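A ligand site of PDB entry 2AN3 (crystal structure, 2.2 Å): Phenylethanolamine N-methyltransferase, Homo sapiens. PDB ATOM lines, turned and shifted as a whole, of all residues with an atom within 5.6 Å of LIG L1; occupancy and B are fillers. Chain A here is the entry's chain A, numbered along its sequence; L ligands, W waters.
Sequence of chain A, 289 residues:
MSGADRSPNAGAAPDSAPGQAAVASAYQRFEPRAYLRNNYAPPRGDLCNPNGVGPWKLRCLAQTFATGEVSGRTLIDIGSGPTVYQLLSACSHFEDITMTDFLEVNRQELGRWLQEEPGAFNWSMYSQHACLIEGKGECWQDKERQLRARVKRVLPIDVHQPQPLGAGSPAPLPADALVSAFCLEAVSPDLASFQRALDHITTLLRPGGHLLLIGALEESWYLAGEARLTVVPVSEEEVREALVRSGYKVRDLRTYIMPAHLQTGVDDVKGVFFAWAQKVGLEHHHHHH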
ATOM      1  N   VAL A  23     -16.262 -11.079 -20.045  1.00  0.00           N
ATOM      2  CA  VAL A  23     -15.617 -10.298 -18.943  1.00  0.00           C
ATOM      3  C   VAL A  23     -15.237  -8.904 -19.433  1.00  0.00           C
ATOM      4  O   VAL A  23     -15.791  -7.907 -18.966  1.00  0.00           O
ATOM      5  CB  VAL A  23     -14.361 -11.024 -18.412  1.00  0.00           C
ATOM      6  CG1 VAL A  23     -13.580 -10.118 -17.467  1.00  0.00           C
ATOM      7  CG2 VAL A  23     -14.755 -12.310 -17.693  1.00  0.00           C
ATOM      8  N   TYR A  27     -16.623  -5.336 -17.750  1.00  0.00           N
ATOM      9  CA  TYR A  27     -15.853  -4.257 -17.137  1.00  0.00           C
ATOM     10  C   TYR A  27     -16.021  -2.908 -17.810  1.00  0.00           C
ATOM     11  O   TYR A  27     -15.572  -1.886 -17.278  1.00  0.00           O
ATOM     12  CB  TYR A  27     -14.373  -4.631 -17.068  1.00  0.00           C
ATOM     13  CG  TYR A  27     -14.055  -5.466 -15.852  1.00  0.00           C
ATOM     14  CD1 TYR A  27     -13.953  -6.860 -15.939  1.00  0.00           C
ATOM     15  CD2 TYR A  27     -13.937  -4.884 -14.591  1.00  0.00           C
ATOM     16  CE1 TYR A  27     -13.744  -7.647 -14.811  1.00  0.00           C
ATOM     17  CE2 TYR A  27     -13.741  -5.664 -13.454  1.00  0.00           C
ATOM     18  CZ  TYR A  27     -13.635  -7.038 -13.572  1.00  0.00           C
ATOM     19  OH  TYR A  27     -13.446  -7.800 -12.448  1.00  0.00           O
ATOM     20  N   PHE A  30     -17.729  -0.732 -15.528  1.00  0.00           N
ATOM     21  CA  PHE A  30     -17.075  -0.623 -14.224  1.00  0.00           C
ATOM     22  C   PHE A  30     -16.944   0.844 -13.803  1.00  0.00           C
ATOM     23  O   PHE A  30     -16.334   1.644 -14.517  1.00  0.00           O
ATOM     24  CB  PHE A  30     -15.685  -1.267 -14.294  1.00  0.00           C
ATOM     25  CG  PHE A  30     -14.948  -1.312 -12.992  1.00  0.00           C
ATOM     26  CD1 PHE A  30     -15.000  -2.442 -12.188  1.00  0.00           C
ATOM     27  CD2 PHE A  30     -14.175  -0.234 -12.577  1.00  0.00           C
ATOM     28  CE1 PHE A  30     -14.291  -2.502 -10.988  1.00  0.00           C
ATOM     29  CE2 PHE A  30     -13.451  -0.278 -11.381  1.00  0.00           C
ATOM     30  CZ  PHE A  30     -13.513  -1.426 -10.587  1.00  0.00           C
ATOM     31  N   TYR A  35     -16.968   1.494  -7.009  1.00  0.00           N
ATOM     32  CA  TYR A  35     -16.133   0.392  -6.534  1.00  0.00           C
ATOM     33  C   TYR A  35     -15.461   0.820  -5.227  1.00  0.00           C
ATOM     34  O   TYR A  35     -15.568   0.136  -4.211  1.00  0.00           O
ATOM     35  CB  TYR A  35     -15.059   0.039  -7.566  1.00  0.00           C
ATOM     36  CG  TYR A  35     -14.115  -1.054  -7.131  1.00  0.00           C
ATOM     37  CD1 TYR A  35     -14.486  -2.397  -7.204  1.00  0.00           C
ATOM     38  CD2 TYR A  35     -12.837  -0.754  -6.660  1.00  0.00           C
ATOM     39  CE1 TYR A  35     -13.616  -3.421  -6.815  1.00  0.00           C
ATOM     40  CE2 TYR A  35     -11.958  -1.767  -6.268  1.00  0.00           C
ATOM     41  CZ  TYR A  35     -12.351  -3.092  -6.352  1.00  0.00           C
ATOM     42  OH  TYR A  35     -11.477  -4.097  -5.994  1.00  0.00           O
ATOM     43  N   TYR A  40     -13.959   0.317  -0.044  1.00  0.00           N
ATOM     44  CA  TYR A  40     -12.969   1.047   0.723  1.00  0.00           C
ATOM     45  C   TYR A  40     -13.488   2.266   1.472  1.00  0.00           C
ATOM     46  O   TYR A  40     -12.740   3.160   1.835  1.00  0.00           O
ATOM     47  CB  TYR A  40     -11.781   1.396  -0.187  1.00  0.00           C
ATOM     48  CG  TYR A  40     -11.162   0.144  -0.753  1.00  0.00           C
ATOM     49  CD1 TYR A  40     -11.511  -0.336  -2.021  1.00  0.00           C
ATOM     50  CD2 TYR A  40     -10.291  -0.636   0.024  1.00  0.00           C
ATOM     51  CE1 TYR A  40     -11.007  -1.547  -2.508  1.00  0.00           C
ATOM     52  CE2 TYR A  40      -9.792  -1.839  -0.443  1.00  0.00           C
ATOM     53  CZ  TYR A  40     -10.153  -2.294  -1.703  1.00  0.00           C
ATOM     54  OH  TYR A  40      -9.651  -3.485  -2.155  1.00  0.00           O
ATOM     55  N   ASP A  77       2.501  -3.960  -9.895  1.00  0.00           N
ATOM     56  CA  ASP A  77       1.219  -4.238  -9.256  1.00  0.00           C
ATOM     57  C   ASP A  77       0.253  -4.578 -10.386  1.00  0.00           C
ATOM     58  O   ASP A  77      -0.057  -3.730 -11.216  1.00  0.00           O
ATOM     59  CB  ASP A  77       0.720  -3.004  -8.469  1.00  0.00           C
ATOM     60  CG  ASP A  77      -0.595  -3.284  -7.742  1.00  0.00           C
ATOM     61  OD1 ASP A  77      -0.758  -4.414  -7.237  1.00  0.00           O
ATOM     62  OD2 ASP A  77      -1.447  -2.374  -7.665  1.00  0.00           O
ATOM     63  N   ILE A  78      -0.185  -5.831 -10.404  1.00  0.00           N
ATOM     64  CA  ILE A  78      -1.077  -6.357 -11.429  1.00  0.00           C
ATOM     65  C   ILE A  78      -2.553  -6.084 -11.146  1.00  0.00           C
ATOM     66  O   ILE A  78      -3.092  -6.548 -10.148  1.00  0.00           O
ATOM     67  CB  ILE A  78      -0.895  -7.886 -11.560  1.00  0.00           C
ATOM     68  CG1 ILE A  78       0.588  -8.233 -11.701  1.00  0.00           C
ATOM     69  CG2 ILE A  78      -1.712  -8.422 -12.723  1.00  0.00           C
ATOM     70  CD1 ILE A  78       1.217  -7.761 -13.001  1.00  0.00           C
ATOM     71  N   GLY A  79      -3.205  -5.343 -12.037  1.00  0.00           N
ATOM     72  CA  GLY A  79      -4.615  -5.054 -11.859  1.00  0.00           C
ATOM     73  C   GLY A  79      -4.887  -4.169 -10.655  1.00  0.00           C
ATOM     74  O   GLY A  79      -5.701  -4.511  -9.792  1.00  0.00           O
ATOM     75  N   SER A  80      -4.210  -3.035 -10.617  1.00  0.00           N
ATOM     76  CA  SER A  80      -4.315  -2.071  -9.538  1.00  0.00           C
ATOM     77  C   SER A  80      -5.706  -1.485  -9.393  1.00  0.00           C
ATOM     78  O   SER A  80      -6.128  -1.131  -8.292  1.00  0.00           O
ATOM     79  CB  SER A  80      -3.321  -0.923  -9.755  1.00  0.00           C
ATOM     80  OG  SER A  80      -2.005  -1.403  -9.911  1.00  0.00           O
ATOM     81  N   GLY A  81      -6.415  -1.371 -10.506  1.00  0.00           N
ATOM     82  CA  GLY A  81      -7.727  -0.759 -10.424  1.00  0.00           C
ATOM     83  C   GLY A  81      -7.519   0.641  -9.879  1.00  0.00           C
ATOM     84  O   GLY A  81      -6.458   1.227 -10.052  1.00  0.00           O
ATOM     85  N   PRO A  82      -8.519   1.214  -9.195  1.00  0.00           N
ATOM     86  CA  PRO A  82      -8.344   2.567  -8.658  1.00  0.00           C
ATOM     87  C   PRO A  82      -7.838   2.616  -7.209  1.00  0.00           C
ATOM     88  O   PRO A  82      -8.099   3.592  -6.510  1.00  0.00           O
ATOM     89  CB  PRO A  82      -9.736   3.145  -8.797  1.00  0.00           C
ATOM     90  CG  PRO A  82     -10.597   1.971  -8.422  1.00  0.00           C
ATOM     91  CD  PRO A  82      -9.936   0.805  -9.150  1.00  0.00           C
ATOM     92  N   THR A  83      -7.103   1.597  -6.760  1.00  0.00           N
ATOM     93  CA  THR A  83      -6.644   1.584  -5.370  1.00  0.00           C
ATOM     94  C   THR A  83      -5.121   1.579  -5.186  1.00  0.00           C
ATOM     95  O   THR A  83      -4.380   1.134  -6.053  1.00  0.00           O
ATOM     96  CB  THR A  83      -7.195   0.361  -4.622  1.00  0.00           C
ATOM     97  OG1 THR A  83      -6.470  -0.806  -5.016  1.00  0.00           O
ATOM     98  CG2 THR A  83      -8.682   0.161  -4.930  1.00  0.00           C
ATOM     99  N   TYR A  85      -3.847   1.057  -1.632  1.00  0.00           N
ATOM    100  CA  TYR A  85      -3.612   0.437  -0.320  1.00  0.00           C
ATOM    101  C   TYR A  85      -2.689  -0.760  -0.390  1.00  0.00           C
ATOM    102  O   TYR A  85      -1.918  -1.015   0.541  1.00  0.00           O
ATOM    103  CB  TYR A  85      -4.944   0.018   0.330  1.00  0.00           C
ATOM    104  CG  TYR A  85      -5.479  -1.295  -0.191  1.00  0.00           C
ATOM    105  CD1 TYR A  85      -5.024  -2.521   0.326  1.00  0.00           C
ATOM    106  CD2 TYR A  85      -6.356  -1.322  -1.273  1.00  0.00           C
ATOM    107  CE1 TYR A  85      -5.424  -3.729  -0.243  1.00  0.00           C
ATOM    108  CE2 TYR A  85      -6.769  -2.522  -1.833  1.00  0.00           C
ATOM    109  CZ  TYR A  85      -6.299  -3.714  -1.321  1.00  0.00           C
ATOM    110  OH  TYR A  85      -6.680  -4.885  -1.925  1.00  0.00           O
ATOM    111  N   GLN A  86      -2.780  -1.524  -1.473  1.00  0.00           N
ATOM    112  CA  GLN A  86      -1.968  -2.707  -1.629  1.00  0.00           C
ATOM    113  C   GLN A  86      -0.466  -2.407  -1.741  1.00  0.00           C
ATOM    114  O   GLN A  86       0.351  -3.323  -1.648  1.00  0.00           O
ATOM    115  CB  GLN A  86      -2.410  -3.510  -2.868  1.00  0.00           C
ATOM    116  CG  GLN A  86      -2.173  -2.815  -4.209  1.00  0.00           C
ATOM    117  CD  GLN A  86      -3.404  -2.076  -4.715  1.00  0.00           C
ATOM    118  OE1 GLN A  86      -4.186  -1.533  -3.937  1.00  0.00           O
ATOM    119  NE2 GLN A  86      -3.581  -2.046  -6.037  1.00  0.00           N
ATOM    120  N   ASP A 101      -3.494  -1.603 -15.027  1.00  0.00           N
ATOM    121  CA  ASP A 101      -4.913  -1.894 -15.096  1.00  0.00           C
ATOM    122  C   ASP A 101      -5.447  -1.920 -16.506  1.00  0.00           C
ATOM    123  O   ASP A 101      -4.926  -1.260 -17.402  1.00  0.00           O
ATOM    124  CB  ASP A 101      -5.758  -0.949 -14.266  1.00  0.00           C
ATOM    125  CG  ASP A 101      -7.068  -1.577 -13.853  1.00  0.00           C
ATOM    126  OD1 ASP A 101      -7.018  -2.591 -13.126  1.00  0.00           O
ATOM    127  OD2 ASP A 101      -8.137  -1.081 -14.273  1.00  0.00           O
ATOM    128  N   PHE A 102      -6.513  -2.694 -16.675  1.00  0.00           N
ATOM    129  CA  PHE A 102      -7.189  -2.881 -17.949  1.00  0.00           C
ATOM    130  C   PHE A 102      -7.956  -1.647 -18.403  1.00  0.00           C
ATOM    131  O   PHE A 102      -7.931  -1.287 -19.579  1.00  0.00           O
ATOM    132  CB  PHE A 102      -8.174  -4.055 -17.817  1.00  0.00           C
ATOM    133  CG  PHE A 102      -8.736  -4.552 -19.125  1.00  0.00           C
ATOM    134  CD1 PHE A 102      -7.963  -5.328 -19.980  1.00  0.00           C
ATOM    135  CD2 PHE A 102     -10.045  -4.255 -19.491  1.00  0.00           C
ATOM    136  CE1 PHE A 102      -8.490  -5.816 -21.182  1.00  0.00           C
ATOM    137  CE2 PHE A 102     -10.579  -4.737 -20.696  1.00  0.00           C
ATOM    138  CZ  PHE A 102      -9.797  -5.523 -21.531  1.00  0.00           C
ATOM    139  N   LEU A 103      -8.640  -1.001 -17.466  1.00  0.00           N
ATOM    140  CA  LEU A 103      -9.454   0.148 -17.799  1.00  0.00           C
ATOM    141  C   LEU A 103      -8.748   1.503 -17.743  1.00  0.00           C
ATOM    142  O   LEU A 103      -7.938   1.759 -16.845  1.00  0.00           O
ATOM    143  CB  LEU A 103     -10.691   0.183 -16.891  1.00  0.00           C
ATOM    144  CG  LEU A 103     -11.533  -1.105 -16.926  1.00  0.00           C
ATOM    145  CD1 LEU A 103     -12.659  -1.012 -15.902  1.00  0.00           C
ATOM    146  CD2 LEU A 103     -12.096  -1.297 -18.322  1.00  0.00           C
ATOM    147  N   ASN A 106      -9.754   3.585 -14.684  1.00  0.00           N
ATOM    148  CA  ASN A 106      -9.065   3.305 -13.437  1.00  0.00           C
ATOM    149  C   ASN A 106      -7.711   3.993 -13.432  1.00  0.00           C
ATOM    150  O   ASN A 106      -7.340   4.670 -12.470  1.00  0.00           O
ATOM    151  CB  ASN A 106      -8.893   1.797 -13.214  1.00  0.00           C
ATOM    152  CG  ASN A 106     -10.125   1.152 -12.628  1.00  0.00           C
ATOM    153  OD1 ASN A 106     -10.862   1.779 -11.864  1.00  0.00           O
ATOM    154  ND2 ASN A 106     -10.364  -0.112 -12.978  1.00  0.00           N
ATOM    155  N   ILE A 157      -2.965  -3.108 -19.040  1.00  0.00           N
ATOM    156  CA  ILE A 157      -2.558  -4.491 -18.925  1.00  0.00           C
ATOM    157  C   ILE A 157      -3.722  -5.437 -19.170  1.00  0.00           C
ATOM    158  O   ILE A 157      -4.878  -5.084 -18.987  1.00  0.00           O
ATOM    159  CB  ILE A 157      -1.957  -4.772 -17.530  1.00  0.00           C
ATOM    160  CG1 ILE A 157      -1.426  -6.203 -17.436  1.00  0.00           C
ATOM    161  CG2 ILE A 157      -3.017  -4.525 -16.450  1.00  0.00           C
ATOM    162  CD1 ILE A 157      -0.697  -6.504 -16.140  1.00  0.00           C
ATOM    163  N   ASP A 158      -3.391  -6.648 -19.613  1.00  0.00           N
ATOM    164  CA  ASP A 158      -4.390  -7.672 -19.873  1.00  0.00           C
ATOM    165  C   ASP A 158      -3.751  -8.988 -19.485  1.00  0.00           C
ATOM    166  O   ASP A 158      -2.887  -9.505 -20.194  1.00  0.00           O
ATOM    167  CB  ASP A 158      -4.762  -7.705 -21.346  1.00  0.00           C
ATOM    168  CG  ASP A 158      -5.929  -8.625 -21.626  1.00  0.00           C
ATOM    169  OD1 ASP A 158      -5.970  -9.728 -21.020  1.00  0.00           O
ATOM    170  OD2 ASP A 158      -6.806  -8.255 -22.437  1.00  0.00           O
ATOM    171  N   VAL A 159      -4.171  -9.543 -18.351  1.00  0.00           N
ATOM    172  CA  VAL A 159      -3.608 -10.795 -17.872  1.00  0.00           C
ATOM    173  C   VAL A 159      -3.906 -11.990 -18.761  1.00  0.00           C
ATOM    174  O   VAL A 159      -3.264 -13.023 -18.642  1.00  0.00           O
ATOM    175  CB  VAL A 159      -4.106 -11.110 -16.450  1.00  0.00           C
ATOM    176  CG1 VAL A 159      -3.662 -10.014 -15.489  1.00  0.00           C
ATOM    177  CG2 VAL A 159      -5.620 -11.251 -16.444  1.00  0.00           C
ATOM    178  N   HIS A 160      -4.872 -11.828 -19.670  1.00  0.00           N
ATOM    179  CA  HIS A 160      -5.236 -12.923 -20.568  1.00  0.00           C
ATOM    180  C   HIS A 160      -4.277 -13.092 -21.737  1.00  0.00           C
ATOM    181  O   HIS A 160      -4.248 -14.151 -22.377  1.00  0.00           O
ATOM    182  CB  HIS A 160      -6.668 -12.725 -21.066  1.00  0.00           C
ATOM    183  CG  HIS A 160      -7.693 -12.758 -19.979  1.00  0.00           C
ATOM    184  ND1 HIS A 160      -7.755 -13.796 -19.065  1.00  0.00           N
ATOM    185  CD2 HIS A 160      -8.678 -11.898 -19.635  1.00  0.00           C
ATOM    186  CE1 HIS A 160      -8.738 -13.562 -18.213  1.00  0.00           C
ATOM    187  NE2 HIS A 160      -9.316 -12.423 -18.540  1.00  0.00           N
ATOM    188  N   ALA A 181      -4.028  -7.759  -6.208  1.00  0.00           N
ATOM    189  CA  ALA A 181      -5.149  -7.926  -5.307  1.00  0.00           C
ATOM    190  C   ALA A 181      -6.500  -7.844  -6.012  1.00  0.00           C
ATOM    191  O   ALA A 181      -6.816  -6.865  -6.675  1.00  0.00           O
ATOM    192  CB  ALA A 181      -5.082  -6.859  -4.214  1.00  0.00           C
ATOM    193  N   PHE A 182      -7.277  -8.916  -5.860  1.00  0.00           N
ATOM    194  CA  PHE A 182      -8.608  -9.020  -6.437  1.00  0.00           C
ATOM    195  C   PHE A 182      -8.672  -8.844  -7.944  1.00  0.00           C
ATOM    196  O   PHE A 182      -9.603  -8.217  -8.460  1.00  0.00           O
ATOM    197  CB  PHE A 182      -9.533  -8.010  -5.755  1.00  0.00           C
ATOM    198  CG  PHE A 182      -9.576  -8.159  -4.264  1.00  0.00           C
ATOM    199  CD1 PHE A 182      -8.904  -7.260  -3.440  1.00  0.00           C
ATOM    200  CD2 PHE A 182     -10.281  -9.211  -3.677  1.00  0.00           C
ATOM    201  CE1 PHE A 182      -8.924  -7.408  -2.048  1.00  0.00           C
ATOM    202  CE2 PHE A 182     -10.303  -9.365  -2.292  1.00  0.00           C
ATOM    203  CZ  PHE A 182      -9.624  -8.461  -1.474  1.00  0.00           C
ATOM    204  N   CYS A 183      -7.702  -9.400  -8.651  1.00  0.00           N
ATOM    205  CA  CYS A 183      -7.703  -9.272 -10.088  1.00  0.00           C
ATOM    206  C   CYS A 183      -8.001 -10.575 -10.820  1.00  0.00           C
ATOM    207  O   CYS A 183      -9.047 -10.714 -11.444  1.00  0.00           O
ATOM    208  CB  CYS A 183      -6.365  -8.728 -10.581  1.00  0.00           C
ATOM    209  SG  CYS A 183      -6.336  -8.485 -12.388  1.00  0.00           S
ATOM    210  N   ALA A 186     -11.234 -12.254 -10.399  1.00  0.00           N
ATOM    211  CA  ALA A 186     -12.288 -11.347 -10.828  1.00  0.00           C
ATOM    212  C   ALA A 186     -12.328 -11.108 -12.340  1.00  0.00           C
ATOM    213  O   ALA A 186     -13.161 -10.338 -12.824  1.00  0.00           O
ATOM    214  CB  ALA A 186     -12.139 -10.009 -10.100  1.00  0.00           C
ATOM    215  N   VAL A 187     -11.432 -11.757 -13.074  1.00  0.00           N
ATOM    216  CA  VAL A 187     -11.389 -11.569 -14.531  1.00  0.00           C
ATOM    217  C   VAL A 187     -11.350 -12.891 -15.306  1.00  0.00           C
ATOM    218  O   VAL A 187     -11.259 -12.892 -16.530  1.00  0.00           O
ATOM    219  CB  VAL A 187     -10.167 -10.739 -14.942  1.00  0.00           C
ATOM    220  CG1 VAL A 187     -10.174  -9.416 -14.200  1.00  0.00           C
ATOM    221  CG2 VAL A 187      -8.877 -11.511 -14.631  1.00  0.00           C
ATOM    222  N   TYR A 222     -19.618  -9.373  -7.808  1.00  0.00           N
ATOM    223  CA  TYR A 222     -19.465  -8.167  -6.995  1.00  0.00           C
ATOM    224  C   TYR A 222     -19.896  -7.019  -7.901  1.00  0.00           C
ATOM    225  O   TYR A 222     -19.760  -7.115  -9.118  1.00  0.00           O
ATOM    226  CB  TYR A 222     -18.028  -8.000  -6.504  1.00  0.00           C
ATOM    227  CG  TYR A 222     -17.048  -7.518  -7.530  1.00  0.00           C
ATOM    228  CD1 TYR A 222     -16.818  -6.160  -7.725  1.00  0.00           C
ATOM    229  CD2 TYR A 222     -16.331  -8.425  -8.317  1.00  0.00           C
ATOM    230  CE1 TYR A 222     -15.908  -5.713  -8.668  1.00  0.00           C
ATOM    231  CE2 TYR A 222     -15.415  -7.991  -9.264  1.00  0.00           C
ATOM    232  CZ  TYR A 222     -15.209  -6.628  -9.431  1.00  0.00           C
ATOM    233  OH  TYR A 222     -14.328  -6.187 -10.377  1.00  0.00           O
HETATM  234  N1  LIG L   1      -6.515  -4.003  -7.093  1.00  0.00           N
HETATM  235  C1  LIG L   1      -7.698  -3.308  -6.613  1.00  0.00           C
HETATM  236  C2  LIG L   1      -8.818  -3.396  -7.666  1.00  0.00           C
HETATM  237  C3  LIG L   1      -9.208  -4.814  -8.123  1.00  0.00           C
HETATM  238  S1  LIG L   1     -10.748  -4.795  -9.100  1.00  0.00           S
HETATM  239  C4  LIG L   1      -8.180  -3.778  -5.222  1.00  0.00           C
HETATM  240  O1  LIG L   1      -7.445  -4.545  -4.563  1.00  0.00           O
HETATM  241  O2  LIG L   1      -9.264  -3.364  -4.785  1.00  0.00           O
HETATM  242  C5  LIG L   1     -10.302  -5.810 -10.556  1.00  0.00           C
HETATM  243  C6  LIG L   1      -9.545  -4.998 -11.572  1.00  0.00           C
HETATM  244  O3  LIG L   1      -9.041  -5.813 -12.665  1.00  0.00           O
HETATM  245  C7  LIG L   1     -10.275  -3.817 -12.213  1.00  0.00           C
HETATM  246  O4  LIG L   1      -9.525  -2.625 -12.012  1.00  0.00           O
HETATM  247  C8  LIG L   1     -10.403  -4.226 -13.673  1.00  0.00           C
HETATM  248  O5  LIG L   1     -10.434  -3.162 -14.605  1.00  0.00           O
HETATM  249  C9  LIG L   1      -9.140  -5.072 -13.865  1.00  0.00           C
HETATM  250  N2  LIG L   1      -9.183  -5.983 -15.004  1.00  0.00           N
HETATM  251  C10 LIG L   1     -10.299  -6.405 -15.772  1.00  0.00           C
HETATM  252  N3  LIG L   1      -9.980  -7.185 -16.768  1.00  0.00           N
HETATM  253  C11 LIG L   1      -8.608  -7.306 -16.657  1.00  0.00           C
HETATM  254  C12 LIG L   1      -7.712  -8.037 -17.467  1.00  0.00           C
HETATM  255  N4  LIG L   1      -8.091  -8.740 -18.538  1.00  0.00           N
HETATM  256  N5  LIG L   1      -6.390  -7.985 -17.150  1.00  0.00           N
HETATM  257  C13 LIG L   1      -6.022  -7.251 -16.064  1.00  0.00           C
HETATM  258  N6  LIG L   1      -6.792  -6.528 -15.217  1.00  0.00           N
HETATM  259  C14 LIG L   1      -8.094  -6.602 -15.585  1.00  0.00           C
HETATM  260  C1  LG2 L   2     -14.023  -8.556  -3.688  1.00  0.00           C
HETATM  261  C2  LG2 L   2     -13.250  -7.953  -4.874  1.00  0.00           C
HETATM  262  C3  LG2 L   2     -13.322  -6.424  -4.828  1.00  0.00           C
HETATM  263  C4  LG2 L   2     -12.596  -5.907  -3.594  1.00  0.00           C
HETATM  264  C5  LG2 L   2     -12.967  -6.671  -2.316  1.00  0.00           C
HETATM  265  C6  LG2 L   2     -12.625  -6.119  -1.082  1.00  0.00           C
HETATM  266  C7  LG2 L   2     -13.600  -7.912  -2.362  1.00  0.00           C
HETATM  267  C8  LG2 L   2     -13.879  -8.591  -1.186  1.00  0.00           C
HETATM  268  C9  LG2 L   2     -13.530  -8.045   0.050  1.00  0.00           C
HETATM  269  C10 LG2 L   2     -12.904  -6.798   0.093  1.00  0.00           C
HETATM  270  O1  LG2 L   2     -15.421  -8.332  -3.883  1.00  0.00           O
HETATM  271  N1  LG2 L   2     -13.827  -8.449  -6.126  1.00  0.00           N
HETATM  272  O   HOH W   1     -10.695  -9.679 -20.524  1.00  0.00           O
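The side-chain hydroxyl of Tyr 35 is in hydrogen-bond range of an oxygen (O2) of LIG L1 (2.6 Å). OH of Tyr 40 is in hydrogen-bond range of O2 of LIG L1 (2.7 Å). The side-chain carboxylate (OD1) of Asp 101 sits at hydrogen-bond distance from an oxygen (O4) of LIG L1 (2.7 Å). OH of Tyr 85 sits at hydrogen-bond distance from O1 of LIG L1 (2.8 Å). ND2 of Asn 106 sits at hydrogen-bond distance from O4 of LIG L1, 2.8 Å away. O of Gly 79 sits at hydrogen-bond distance from N1 of LIG L1 (2.9 Å). O of Ala 181 is in hydrogen-bond range of N1 of LIG L1, at 2.9 Å. The backbone NH (N) of Val 159 lies within hydrogen-bond range of a nitrogen (N5) of LIG L1. The backbone carbonyl oxygen (O) of Ser 80 sits at hydrogen-bond distance from a nitrogen (N1) of LIG L1 (3.1 Å). The side-chain carboxylate (OD1) of Asp 158 sits at hydrogen-bond distance from a nitrogen (N4) of LIG L1 (3.4 Å). SG of Cys 183 is in hydrogen-bond range of N6 of LIG L1 (3.5 Å).
The side-chain hydroxyl (OH) of Tyr 85 sits close to the side-chain hydroxyl (OH) of Tyr 40, 3.3 Å away. The side-chain carboxylate (OD2) of Asp 101 lies within hydrogen-bond range of the side-chain amide nitrogen (ND2) of Asn 106, 2.8 Å away. The side-chain carboxylate (OD1) of Asp 101 is in hydrogen-bond range of the backbone NH (N) of Gly 81, at 3.0 Å. N of Ile 157 lies within hydrogen-bond range of O of Asp 101 (3.2 Å). The side-chain hydroxyl of Ser 80 lies within hydrogen-bond range of the side-chain carboxylate of Asp 77 (2.5 Å). OG1 of Thr 83 sits at hydrogen-bond distance from OE1 of Gln 86 (2.6 Å). The backbone carbonyl oxygen (O) of Val 187 lies within hydrogen-bond range of a ring nitrogen (NE2) of His 160 (2.8 Å). The side-chain hydroxyl of Tyr 27 is in hydrogen-bond range of the backbone carbonyl oxygen of Ala 186 (2.6 Å).
A sulfur (S1) of LIG L1 lies close to the backbone carbonyl oxygen of Phe 182 (3.7 Å). Tyr 27 touches LIG L1. CA of Gly 81 touches O4 of LIG L1, 3.0 Å away. Thr 83 touches LIG L1. Gln 86 touches LIG L1 (NE2 to N1, 3.7 Å). Phe 102 touches LIG L1. CG of Leu 103 touches O5 of LIG L1, 3.3 Å away. Ile 157 touches LIG L1. CD2 of His 160 touches N4 of LIG L1 (3.4 Å). CG1 of Val 187 touches C10 of LIG L1 (3.4 Å). Hydrophobic or aromatic side chains within 4 Å of LIG L1: Tyr 27, Tyr 35, Tyr 40, Tyr 85, Phe 102, Leu 103, Val 159, His 160, Ala 181, Phe 182 and Val 187. Within 4 Å of LIG L1: Tyr 27, Tyr 35, Tyr 40, Gly 79, Ser 80, Gly 81, Thr 83, Tyr 85, Gln 86, Asp 101, Phe 102, Leu 103, Asn 106, Ile 157, Asp 158, Val 159, His 160, Ala 181, Phe 182, Cys 183 and Val 187. The nearest printed residue that does not touch LIG L1 is Tyr 222 (4.05 Å).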
